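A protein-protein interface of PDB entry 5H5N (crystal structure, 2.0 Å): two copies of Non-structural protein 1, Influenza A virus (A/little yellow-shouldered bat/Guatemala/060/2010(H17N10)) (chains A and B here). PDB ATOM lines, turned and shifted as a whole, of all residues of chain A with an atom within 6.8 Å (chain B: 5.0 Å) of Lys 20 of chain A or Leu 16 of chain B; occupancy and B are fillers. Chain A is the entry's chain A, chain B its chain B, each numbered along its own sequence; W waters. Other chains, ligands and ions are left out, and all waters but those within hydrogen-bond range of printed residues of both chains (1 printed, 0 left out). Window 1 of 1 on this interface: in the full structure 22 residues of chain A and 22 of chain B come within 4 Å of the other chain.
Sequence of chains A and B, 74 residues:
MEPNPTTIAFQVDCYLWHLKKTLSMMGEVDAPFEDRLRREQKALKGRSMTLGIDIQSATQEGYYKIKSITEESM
Lys 20 of chain A touches one residue of chain B.
Leu 16 of chain B touches one residue of chain A.
Of the printed residues of chain A, Asp 13 of chain B touches Phe 33 and Arg 36.
Of the printed residues of chain B, Leu 19 of chain A touches Ile 66 (3.8 Å).
Of the printed residues of chain A, Lys 20 of chain B touches Leu 16.
Of the printed residues of chain B, Leu 16 of chain A touches Lys 20 (3.6 Å).
Of the printed residues of chain A, Val 12 of chain B touches Leu 23.
The nearest printed residue of chain A that does not touch Lys 20 of chain B is Asp 13 of chain A (4.2 Å).
Among the printed residues, merely in contact across the chains: Phe 33 of chain A with Asp 13 of chain B (3.3 Å), Lys 20 of chain A with Leu 16 of chain B (3.5 Å), Leu 23 of chain A with Val 12 of chain B (3.5 Å), Leu 16 of chain A with Lys 20 of chain B (3.6 Å) and Leu 19 of chain A with Ile 66 of chain B (3.8 Å).
The side-chain amino group of Lys 20 of chain A lies within salt-bridge range of the side-chain carboxylate of Glu 40 of chain A (3.2 Å).
NH2 of Arg 36 of chain A lies within salt-bridge range of OD2 of Asp 13 of chain B (3.0 Å).
Leu 16 of chain A touches Lys 20 of chain B, and with the chains exchanged Lys 20 of chain A touches Leu 16 of chain B.
Positions printed for both chains: 13, 15, 16, 17, 18, 19 and 20.
Water W1 lies within hydrogen-bond range of OD1 of Asp 13 of chain B and NE of Arg 36 of chain A.
Hydrophobic or aromatic side chains of chain A within 4 Å of the printed part of chain B: Leu 16, Leu 19, Leu 23 and Phe 33.
Printed residues of chain B that touch a printed residue of chain A: Val 12, Asp 13, Leu 16, Lys 20 and Ile 66.
Hydrophobic or aromatic side chains of chain B that line the printed part of chain A: Val 12, Leu 16 and Ile 66.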
ATOM      1  N   ASP A  13      -6.133 -21.421  -1.871  1.00  0.00           N
ATOM      2  CA  ASP A  13      -5.097 -21.410  -2.900  1.00  0.00           C
ATOM      3  C   ASP A  13      -5.583 -22.102  -4.173  1.00  0.00           C
ATOM      4  O   ASP A  13      -5.343 -21.615  -5.285  1.00  0.00           O
ATOM      5  CB  ASP A  13      -3.779 -22.024  -2.423  1.00  0.00           C
ATOM      6  CG  ASP A  13      -2.964 -21.084  -1.543  1.00  0.00           C
ATOM      7  OD1 ASP A  13      -3.179 -19.850  -1.555  1.00  0.00           O
ATOM      8  OD2 ASP A  13      -2.070 -21.595  -0.853  1.00  0.00           O
ATOM      9  N   TYR A  15      -8.790 -22.464  -5.191  1.00  0.00           N
ATOM     10  CA  TYR A  15      -9.760 -21.602  -5.875  1.00  0.00           C
ATOM     11  C   TYR A  15      -9.112 -20.415  -6.629  1.00  0.00           C
ATOM     12  O   TYR A  15      -9.428 -20.123  -7.809  1.00  0.00           O
ATOM     13  CB  TYR A  15     -10.863 -21.110  -4.925  1.00  0.00           C
ATOM     14  CG  TYR A  15     -11.845 -20.202  -5.621  1.00  0.00           C
ATOM     15  CD1 TYR A  15     -12.569 -20.653  -6.706  1.00  0.00           C
ATOM     16  CD2 TYR A  15     -12.024 -18.890  -5.214  1.00  0.00           C
ATOM     17  CE1 TYR A  15     -13.465 -19.830  -7.364  1.00  0.00           C
ATOM     18  CE2 TYR A  15     -12.921 -18.054  -5.864  1.00  0.00           C
ATOM     19  CZ  TYR A  15     -13.637 -18.534  -6.944  1.00  0.00           C
ATOM     20  OH  TYR A  15     -14.528 -17.728  -7.618  1.00  0.00           O
ATOM     21  N   LEU A  16      -8.198 -19.729  -5.956  1.00  0.00           N
ATOM     22  CA  LEU A  16      -7.551 -18.583  -6.578  1.00  0.00           C
ATOM     23  C   LEU A  16      -6.704 -19.009  -7.795  1.00  0.00           C
ATOM     24  O   LEU A  16      -6.617 -18.280  -8.800  1.00  0.00           O
ATOM     25  CB  LEU A  16      -6.737 -17.795  -5.548  1.00  0.00           C
ATOM     26  CG  LEU A  16      -7.570 -17.238  -4.377  1.00  0.00           C
ATOM     27  CD1 LEU A  16      -6.692 -16.372  -3.491  1.00  0.00           C
ATOM     28  CD2 LEU A  16      -8.782 -16.467  -4.827  1.00  0.00           C
ATOM     29  N   TRP A  17      -6.103 -20.197  -7.714  1.00  0.00           N
ATOM     30  CA  TRP A  17      -5.392 -20.731  -8.877  1.00  0.00           C
ATOM     31  C   TRP A  17      -6.375 -20.968 -10.016  1.00  0.00           C
ATOM     32  O   TRP A  17      -6.079 -20.656 -11.155  1.00  0.00           O
ATOM     33  CB  TRP A  17      -4.615 -22.006  -8.575  1.00  0.00           C
ATOM     34  CG  TRP A  17      -3.777 -22.462  -9.775  1.00  0.00           C
ATOM     35  CD1 TRP A  17      -2.481 -22.109 -10.057  1.00  0.00           C
ATOM     36  CD2 TRP A  17      -4.205 -23.312 -10.849  1.00  0.00           C
ATOM     37  NE1 TRP A  17      -2.075 -22.708 -11.230  1.00  0.00           N
ATOM     38  CE2 TRP A  17      -3.112 -23.452 -11.733  1.00  0.00           C
ATOM     39  CE3 TRP A  17      -5.401 -23.989 -11.140  1.00  0.00           C
ATOM     40  CZ2 TRP A  17      -3.181 -24.223 -12.889  1.00  0.00           C
ATOM     41  CZ3 TRP A  17      -5.471 -24.758 -12.289  1.00  0.00           C
ATOM     42  CH2 TRP A  17      -4.365 -24.869 -13.155  1.00  0.00           C
ATOM     43  N   HIS A  18      -7.538 -21.530  -9.703  1.00  0.00           N
ATOM     44  CA  HIS A  18      -8.585 -21.709 -10.718  1.00  0.00           C
ATOM     45  C   HIS A  18      -8.954 -20.408 -11.434  1.00  0.00           C
ATOM     46  O   HIS A  18      -9.123 -20.384 -12.669  1.00  0.00           O
ATOM     47  CB  HIS A  18      -9.816 -22.373 -10.086  1.00  0.00           C
ATOM     48  CG  HIS A  18     -11.056 -22.256 -10.909  1.00  0.00           C
ATOM     49  ND1 HIS A  18     -11.294 -23.040 -12.013  1.00  0.00           N
ATOM     50  CD2 HIS A  18     -12.140 -21.459 -10.767  1.00  0.00           C
ATOM     51  CE1 HIS A  18     -12.472 -22.720 -12.531  1.00  0.00           C
ATOM     52  NE2 HIS A  18     -13.005 -21.767 -11.787  1.00  0.00           N
ATOM     53  N   LEU A  19      -9.081 -19.325 -10.668  1.00  0.00           N
ATOM     54  CA  LEU A  19      -9.338 -18.006 -11.273  1.00  0.00           C
ATOM     55  C   LEU A  19      -8.194 -17.544 -12.182  1.00  0.00           C
ATOM     56  O   LEU A  19      -8.421 -17.006 -13.301  1.00  0.00           O
ATOM     57  CB  LEU A  19      -9.606 -16.945 -10.207  1.00  0.00           C
ATOM     58  CG  LEU A  19     -10.826 -17.148  -9.315  1.00  0.00           C
ATOM     59  CD1 LEU A  19     -10.903 -16.026  -8.305  1.00  0.00           C
ATOM     60  CD2 LEU A  19     -12.079 -17.140 -10.153  1.00  0.00           C
ATOM     61  N   LYS A  20      -6.962 -17.731 -11.712  1.00  0.00           N
ATOM     62  CA  LYS A  20      -5.823 -17.307 -12.529  1.00  0.00           C
ATOM     63  C   LYS A  20      -5.703 -18.119 -13.835  1.00  0.00           C
ATOM     64  O   LYS A  20      -5.389 -17.571 -14.901  1.00  0.00           O
ATOM     65  CB  LYS A  20      -4.526 -17.322 -11.708  1.00  0.00           C
ATOM     66  CG  LYS A  20      -4.550 -16.291 -10.560  1.00  0.00           C
ATOM     67  CD  LYS A  20      -3.210 -16.145  -9.805  1.00  0.00           C
ATOM     68  CE  LYS A  20      -2.946 -17.328  -8.910  1.00  0.00           C
ATOM     69  NZ  LYS A  20      -2.019 -17.002  -7.768  1.00  0.00           N
ATOM     70  N   LYS A  21      -5.958 -19.423 -13.739  1.00  0.00           N
ATOM     71  CA  LYS A  21      -5.925 -20.315 -14.888  1.00  0.00           C
ATOM     72  C   LYS A  21      -7.031 -19.924 -15.865  1.00  0.00           C
ATOM     73  O   LYS A  21      -6.818 -19.900 -17.078  1.00  0.00           O
ATOM     74  CB  LYS A  21      -6.059 -21.783 -14.457  1.00  0.00           C
ATOM     75  CG  LYS A  21      -6.047 -22.784 -15.624  1.00  0.00           C
ATOM     76  CD  LYS A  21      -4.702 -22.818 -16.351  1.00  0.00           C
ATOM     77  CE  LYS A  21      -4.691 -23.924 -17.427  1.00  0.00           C
ATOM     78  NZ  LYS A  21      -3.426 -23.930 -18.260  1.00  0.00           N
ATOM     79  N   THR A  22      -8.201 -19.597 -15.320  1.00  0.00           N
ATOM     80  CA  THR A  22      -9.310 -19.086 -16.129  1.00  0.00           C
ATOM     81  C   THR A  22      -8.868 -17.861 -16.927  1.00  0.00           C
ATOM     82  O   THR A  22      -9.054 -17.800 -18.147  1.00  0.00           O
ATOM     83  CB  THR A  22     -10.548 -18.722 -15.268  1.00  0.00           C
ATOM     84  OG1 THR A  22     -11.094 -19.902 -14.673  1.00  0.00           O
ATOM     85  CG2 THR A  22     -11.620 -18.060 -16.131  1.00  0.00           C
ATOM     86  N   LEU A  23      -8.247 -16.897 -16.256  1.00  0.00           N
ATOM     87  CA  LEU A  23      -7.740 -15.738 -16.989  1.00  0.00           C
ATOM     88  C   LEU A  23      -6.689 -16.070 -18.048  1.00  0.00           C
ATOM     89  O   LEU A  23      -6.658 -15.442 -19.120  1.00  0.00           O
ATOM     90  CB  LEU A  23      -7.207 -14.674 -16.052  1.00  0.00           C
ATOM     91  CG  LEU A  23      -8.339 -13.971 -15.309  1.00  0.00           C
ATOM     92  CD1 LEU A  23      -7.779 -13.326 -14.082  1.00  0.00           C
ATOM     93  CD2 LEU A  23      -8.990 -12.934 -16.228  1.00  0.00           C
ATOM     94  N   SER A  24      -5.820 -17.032 -17.750  1.00  0.00           N
ATOM     95  CA  SER A  24      -4.811 -17.416 -18.727  1.00  0.00           C
ATOM     96  C   SER A  24      -5.437 -18.034 -19.966  1.00  0.00           C
ATOM     97  O   SER A  24      -5.003 -17.766 -21.092  1.00  0.00           O
ATOM     98  CB  SER A  24      -3.806 -18.397 -18.135  1.00  0.00           C
ATOM     99  OG  SER A  24      -2.881 -18.799 -19.132  1.00  0.00           O
ATOM    100  N   MET A  25      -6.450 -18.868 -19.739  1.00  0.00           N
ATOM    101  CA  MET A  25      -7.171 -19.552 -20.808  1.00  0.00           C
ATOM    102  C   MET A  25      -7.908 -18.574 -21.713  1.00  0.00           C
ATOM    103  O   MET A  25      -8.160 -18.875 -22.880  1.00  0.00           O
ATOM    104  CB  MET A  25      -8.159 -20.564 -20.221  1.00  0.00           C
ATOM    105  CG  MET A  25      -7.518 -21.853 -19.710  1.00  0.00           C
ATOM    106  SD  MET A  25      -8.708 -22.929 -18.872  1.00  0.00           S
ATOM    107  CE  MET A  25     -10.235 -22.420 -19.654  1.00  0.00           C
ATOM    108  N   VAL A  29      -3.618 -12.475 -19.725  1.00  0.00           N
ATOM    109  CA  VAL A  29      -2.471 -12.205 -18.845  1.00  0.00           C
ATOM    110  C   VAL A  29      -1.137 -12.413 -19.553  1.00  0.00           C
ATOM    111  O   VAL A  29      -1.088 -13.046 -20.614  1.00  0.00           O
ATOM    112  CB  VAL A  29      -2.525 -13.069 -17.564  1.00  0.00           C
ATOM    113  CG1 VAL A  29      -3.642 -12.589 -16.653  1.00  0.00           C
ATOM    114  CG2 VAL A  29      -2.778 -14.504 -17.924  1.00  0.00           C
ATOM    115  N   PHE A  33       3.134 -14.063 -15.570  1.00  0.00           N
ATOM    116  CA  PHE A  33       1.953 -14.528 -14.833  1.00  0.00           C
ATOM    117  C   PHE A  33       1.703 -16.011 -15.112  1.00  0.00           C
ATOM    118  O   PHE A  33       1.401 -16.779 -14.201  1.00  0.00           O
ATOM    119  CB  PHE A  33       0.721 -13.680 -15.216  1.00  0.00           C
ATOM    120  CG  PHE A  33      -0.560 -14.004 -14.442  1.00  0.00           C
ATOM    121  CD1 PHE A  33      -0.969 -13.208 -13.375  1.00  0.00           C
ATOM    122  CD2 PHE A  33      -1.388 -15.051 -14.834  1.00  0.00           C
ATOM    123  CE1 PHE A  33      -2.165 -13.476 -12.697  1.00  0.00           C
ATOM    124  CE2 PHE A  33      -2.579 -15.331 -14.165  1.00  0.00           C
ATOM    125  CZ  PHE A  33      -2.977 -14.538 -13.109  1.00  0.00           C
ATOM    126  N   GLU A  34       1.829 -16.420 -16.373  1.00  0.00           N
ATOM    127  CA  GLU A  34       1.612 -17.813 -16.756  1.00  0.00           C
ATOM    128  C   GLU A  34       2.703 -18.769 -16.257  1.00  0.00           C
ATOM    129  O   GLU A  34       2.421 -19.895 -15.860  1.00  0.00           O
ATOM    130  CB  GLU A  34       1.385 -17.911 -18.281  1.00  0.00           C
ATOM    131  CG  GLU A  34       0.027 -17.310 -18.652  1.00  0.00           C
ATOM    132  CD  GLU A  34      -0.203 -17.142 -20.151  1.00  0.00           C
ATOM    133  OE1 GLU A  34       0.783 -16.992 -20.903  1.00  0.00           O
ATOM    134  OE2 GLU A  34      -1.390 -17.182 -20.563  1.00  0.00           O
ATOM    135  N   ARG A  36       4.377 -18.223 -13.475  1.00  0.00           N
ATOM    136  CA  ARG A  36       3.985 -18.340 -12.060  1.00  0.00           C
ATOM    137  C   ARG A  36       2.857 -19.346 -11.901  1.00  0.00           C
ATOM    138  O   ARG A  36       2.871 -20.196 -11.016  1.00  0.00           O
ATOM    139  CB  ARG A  36       3.545 -16.987 -11.465  1.00  0.00           C
ATOM    140  CG  ARG A  36       4.670 -15.970 -11.291  1.00  0.00           C
ATOM    141  CD  ARG A  36       4.219 -14.785 -10.400  1.00  0.00           C
ATOM    142  NE  ARG A  36       3.236 -13.877 -11.010  1.00  0.00           N
ATOM    143  CZ  ARG A  36       3.528 -12.949 -11.918  1.00  0.00           C
ATOM    144  NH1 ARG A  36       4.762 -12.835 -12.385  1.00  0.00           N
ATOM    145  NH2 ARG A  36       2.576 -12.153 -12.383  1.00  0.00           N
ATOM    146  N   LEU A  37       1.878 -19.256 -12.786  1.00  0.00           N
ATOM    147  CA  LEU A  37       0.722 -20.146 -12.763  1.00  0.00           C
ATOM    148  C   LEU A  37       1.116 -21.620 -12.885  1.00  0.00           C
ATOM    149  O   LEU A  37       0.578 -22.480 -12.191  1.00  0.00           O
ATOM    150  CB  LEU A  37      -0.245 -19.770 -13.900  1.00  0.00           C
ATOM    151  CG  LEU A  37      -1.599 -20.493 -13.993  1.00  0.00           C
ATOM    152  CD1 LEU A  37      -2.563 -19.999 -12.902  1.00  0.00           C
ATOM    153  CD2 LEU A  37      -2.212 -20.319 -15.381  1.00  0.00           C
ATOM    154  N   GLU A  40       2.938 -22.801  -9.736  1.00  0.00           N
ATOM    155  CA  GLU A  40       1.882 -22.940  -8.732  1.00  0.00           C
ATOM    156  C   GLU A  40       1.035 -24.201  -8.933  1.00  0.00           C
ATOM    157  O   GLU A  40       0.630 -24.841  -7.955  1.00  0.00           O
ATOM    158  CB  GLU A  40       1.014 -21.663  -8.683  1.00  0.00           C
ATOM    159  CG  GLU A  40       1.744 -20.458  -8.054  1.00  0.00           C
ATOM    160  CD  GLU A  40       1.201 -19.043  -8.422  1.00  0.00           C
ATOM    161  OE1 GLU A  40       0.208 -18.874  -9.197  1.00  0.00           O
ATOM    162  OE2 GLU A  40       1.812 -18.073  -7.903  1.00  0.00           O
ATOM    163  N   VAL B  12      -5.006  -8.169 -11.261  1.00  0.00           N
ATOM    164  CA  VAL B  12      -5.517  -9.410 -10.699  1.00  0.00           C
ATOM    165  C   VAL B  12      -4.676  -9.853  -9.499  1.00  0.00           C
ATOM    166  O   VAL B  12      -5.226 -10.201  -8.460  1.00  0.00           O
ATOM    167  CB  VAL B  12      -5.601 -10.531 -11.757  1.00  0.00           C
ATOM    168  CG1 VAL B  12      -5.841 -11.884 -11.098  1.00  0.00           C
ATOM    169  CG2 VAL B  12      -6.705 -10.222 -12.762  1.00  0.00           C
ATOM    170  N   ASP B  13      -3.350  -9.793  -9.638  1.00  0.00           N
ATOM    171  CA  ASP B  13      -2.458 -10.182  -8.540  1.00  0.00           C
ATOM    172  C   ASP B  13      -2.704  -9.345  -7.288  1.00  0.00           C
ATOM    173  O   ASP B  13      -2.728  -9.885  -6.179  1.00  0.00           O
ATOM    174  CB  ASP B  13      -0.970 -10.114  -8.945  1.00  0.00           C
ATOM    175  CG  ASP B  13      -0.509 -11.324  -9.781  1.00  0.00           C
ATOM    176  OD1 ASP B  13      -1.121 -12.416  -9.729  1.00  0.00           O
ATOM    177  OD2 ASP B  13       0.490 -11.169 -10.514  1.00  0.00           O
ATOM    178  N   CYS B  14      -2.900  -8.034  -7.470  1.00  0.00           N
ATOM    179  CA  CYS B  14      -3.173  -7.142  -6.346  1.00  0.00           C
ATOM    180  C   CYS B  14      -4.480  -7.482  -5.638  1.00  0.00           C
ATOM    181  O   CYS B  14      -4.531  -7.591  -4.407  1.00  0.00           O
ATOM    182  CB  CYS B  14      -3.166  -5.672  -6.789  1.00  0.00           C
ATOM    183  SG  CYS B  14      -1.511  -4.981  -7.137  1.00  0.00           S
ATOM    184  N   TYR B  15      -5.534  -7.668  -6.417  1.00  0.00           N
ATOM    185  CA  TYR B  15      -6.816  -8.047  -5.834  1.00  0.00           C
ATOM    186  C   TYR B  15      -6.755  -9.371  -5.074  1.00  0.00           C
ATOM    187  O   TYR B  15      -7.266  -9.497  -3.951  1.00  0.00           O
ATOM    188  CB  TYR B  15      -7.926  -8.086  -6.886  1.00  0.00           C
ATOM    189  CG  TYR B  15      -9.247  -8.495  -6.280  1.00  0.00           C
ATOM    190  CD1 TYR B  15      -9.800  -7.762  -5.246  1.00  0.00           C
ATOM    191  CD2 TYR B  15      -9.920  -9.618  -6.720  1.00  0.00           C
ATOM    192  CE1 TYR B  15     -11.008  -8.128  -4.666  1.00  0.00           C
ATOM    193  CE2 TYR B  15     -11.135  -9.995  -6.151  1.00  0.00           C
ATOM    194  CZ  TYR B  15     -11.665  -9.238  -5.119  1.00  0.00           C
ATOM    195  OH  TYR B  15     -12.855  -9.593  -4.533  1.00  0.00           O
ATOM    196  N   LEU B  16      -6.147 -10.374  -5.699  1.00  0.00           N
ATOM    197  CA  LEU B  16      -6.066 -11.690  -5.068  1.00  0.00           C
ATOM    198  C   LEU B  16      -5.211 -11.645  -3.800  1.00  0.00           C
ATOM    199  O   LEU B  16      -5.515 -12.330  -2.806  1.00  0.00           O
ATOM    200  CB  LEU B  16      -5.562 -12.752  -6.062  1.00  0.00           C
ATOM    201  CG  LEU B  16      -6.423 -12.944  -7.324  1.00  0.00           C
ATOM    202  CD1 LEU B  16      -5.865 -14.125  -8.123  1.00  0.00           C
ATOM    203  CD2 LEU B  16      -7.877 -13.180  -7.017  1.00  0.00           C
ATOM    204  N   TRP B  17      -4.155 -10.825  -3.823  1.00  0.00           N
ATOM    205  CA  TRP B  17      -3.373 -10.622  -2.609  1.00  0.00           C
ATOM    206  C   TRP B  17      -4.271 -10.011  -1.528  1.00  0.00           C
ATOM    207  O   TRP B  17      -4.207 -10.397  -0.375  1.00  0.00           O
ATOM    208  CB  TRP B  17      -2.147  -9.734  -2.841  1.00  0.00           C
ATOM    209  CG  TRP B  17      -1.224  -9.649  -1.623  1.00  0.00           C
ATOM    210  CD1 TRP B  17      -0.147 -10.450  -1.353  1.00  0.00           C
ATOM    211  CD2 TRP B  17      -1.336  -8.739  -0.507  1.00  0.00           C
ATOM    212  NE1 TRP B  17       0.429 -10.078  -0.157  1.00  0.00           N
ATOM    213  CE2 TRP B  17      -0.286  -9.041   0.385  1.00  0.00           C
ATOM    214  CE3 TRP B  17      -2.213  -7.702  -0.182  1.00  0.00           C
ATOM    215  CZ2 TRP B  17      -0.094  -8.343   1.582  1.00  0.00           C
ATOM    216  CZ3 TRP B  17      -2.028  -7.015   1.000  1.00  0.00           C
ATOM    217  CH2 TRP B  17      -0.968  -7.330   1.868  1.00  0.00           C
ATOM    218  N   HIS B  18      -5.091  -9.040  -1.911  1.00  0.00           N
ATOM    219  CA  HIS B  18      -6.048  -8.432  -0.977  1.00  0.00           C
ATOM    220  C   HIS B  18      -6.992  -9.457  -0.320  1.00  0.00           C
ATOM    221  O   HIS B  18      -7.218  -9.425   0.892  1.00  0.00           O
ATOM    222  CB  HIS B  18      -6.847  -7.343  -1.691  1.00  0.00           C
ATOM    223  CG  HIS B  18      -7.997  -6.819  -0.891  1.00  0.00           C
ATOM    224  ND1 HIS B  18      -7.842  -5.886   0.108  1.00  0.00           N
ATOM    225  CD2 HIS B  18      -9.321  -7.101  -0.943  1.00  0.00           C
ATOM    226  CE1 HIS B  18      -9.016  -5.609   0.640  1.00  0.00           C
ATOM    227  NE2 HIS B  18      -9.936  -6.334   0.017  1.00  0.00           N
ATOM    228  N   LEU B  19      -7.523 -10.385  -1.111  1.00  0.00           N
ATOM    229  CA  LEU B  19      -8.358 -11.457  -0.550  1.00  0.00           C
ATOM    230  C   LEU B  19      -7.580 -12.326   0.433  1.00  0.00           C
ATOM    231  O   LEU B  19      -8.077 -12.667   1.529  1.00  0.00           O
ATOM    232  CB  LEU B  19      -8.932 -12.339  -1.657  1.00  0.00           C
ATOM    233  CG  LEU B  19      -9.853 -11.682  -2.669  1.00  0.00           C
ATOM    234  CD1 LEU B  19     -10.298 -12.721  -3.672  1.00  0.00           C
ATOM    235  CD2 LEU B  19     -11.049 -11.094  -1.955  1.00  0.00           C
ATOM    236  N   LYS B  20      -6.358 -12.693   0.054  1.00  0.00           N
ATOM    237  CA  LYS B  20      -5.547 -13.531   0.943  1.00  0.00           C
ATOM    238  C   LYS B  20      -5.183 -12.803   2.249  1.00  0.00           C
ATOM    239  O   LYS B  20      -5.198 -13.396   3.338  1.00  0.00           O
ATOM    240  CB  LYS B  20      -4.293 -14.063   0.232  1.00  0.00           C
ATOM    241  CG  LYS B  20      -4.595 -15.041  -0.911  1.00  0.00           C
ATOM    242  CD  LYS B  20      -3.300 -15.686  -1.432  1.00  0.00           C
ATOM    243  CE  LYS B  20      -2.466 -14.703  -2.240  1.00  0.00           C
ATOM    244  NZ  LYS B  20      -1.542 -15.380  -3.221  1.00  0.00           N
ATOM    245  N   ILE B  66     -12.086  -9.858 -11.780  1.00  0.00           N
ATOM    246  CA  ILE B  66     -12.514 -11.113 -11.175  1.00  0.00           C
ATOM    247  C   ILE B  66     -14.040 -11.193 -11.133  1.00  0.00           C
ATOM    248  O   ILE B  66     -14.619 -12.225 -11.461  1.00  0.00           O
ATOM    249  CB  ILE B  66     -11.888 -11.344  -9.774  1.00  0.00           C
ATOM    250  CG1 ILE B  66     -10.369 -11.448  -9.901  1.00  0.00           C
ATOM    251  CG2 ILE B  66     -12.441 -12.616  -9.149  1.00  0.00           C
ATOM    252  CD1 ILE B  66      -9.912 -12.613 -10.761  1.00  0.00           C
HETATM  253  O   HOH W   1       0.436 -14.497 -10.220  1.00  0.00           O
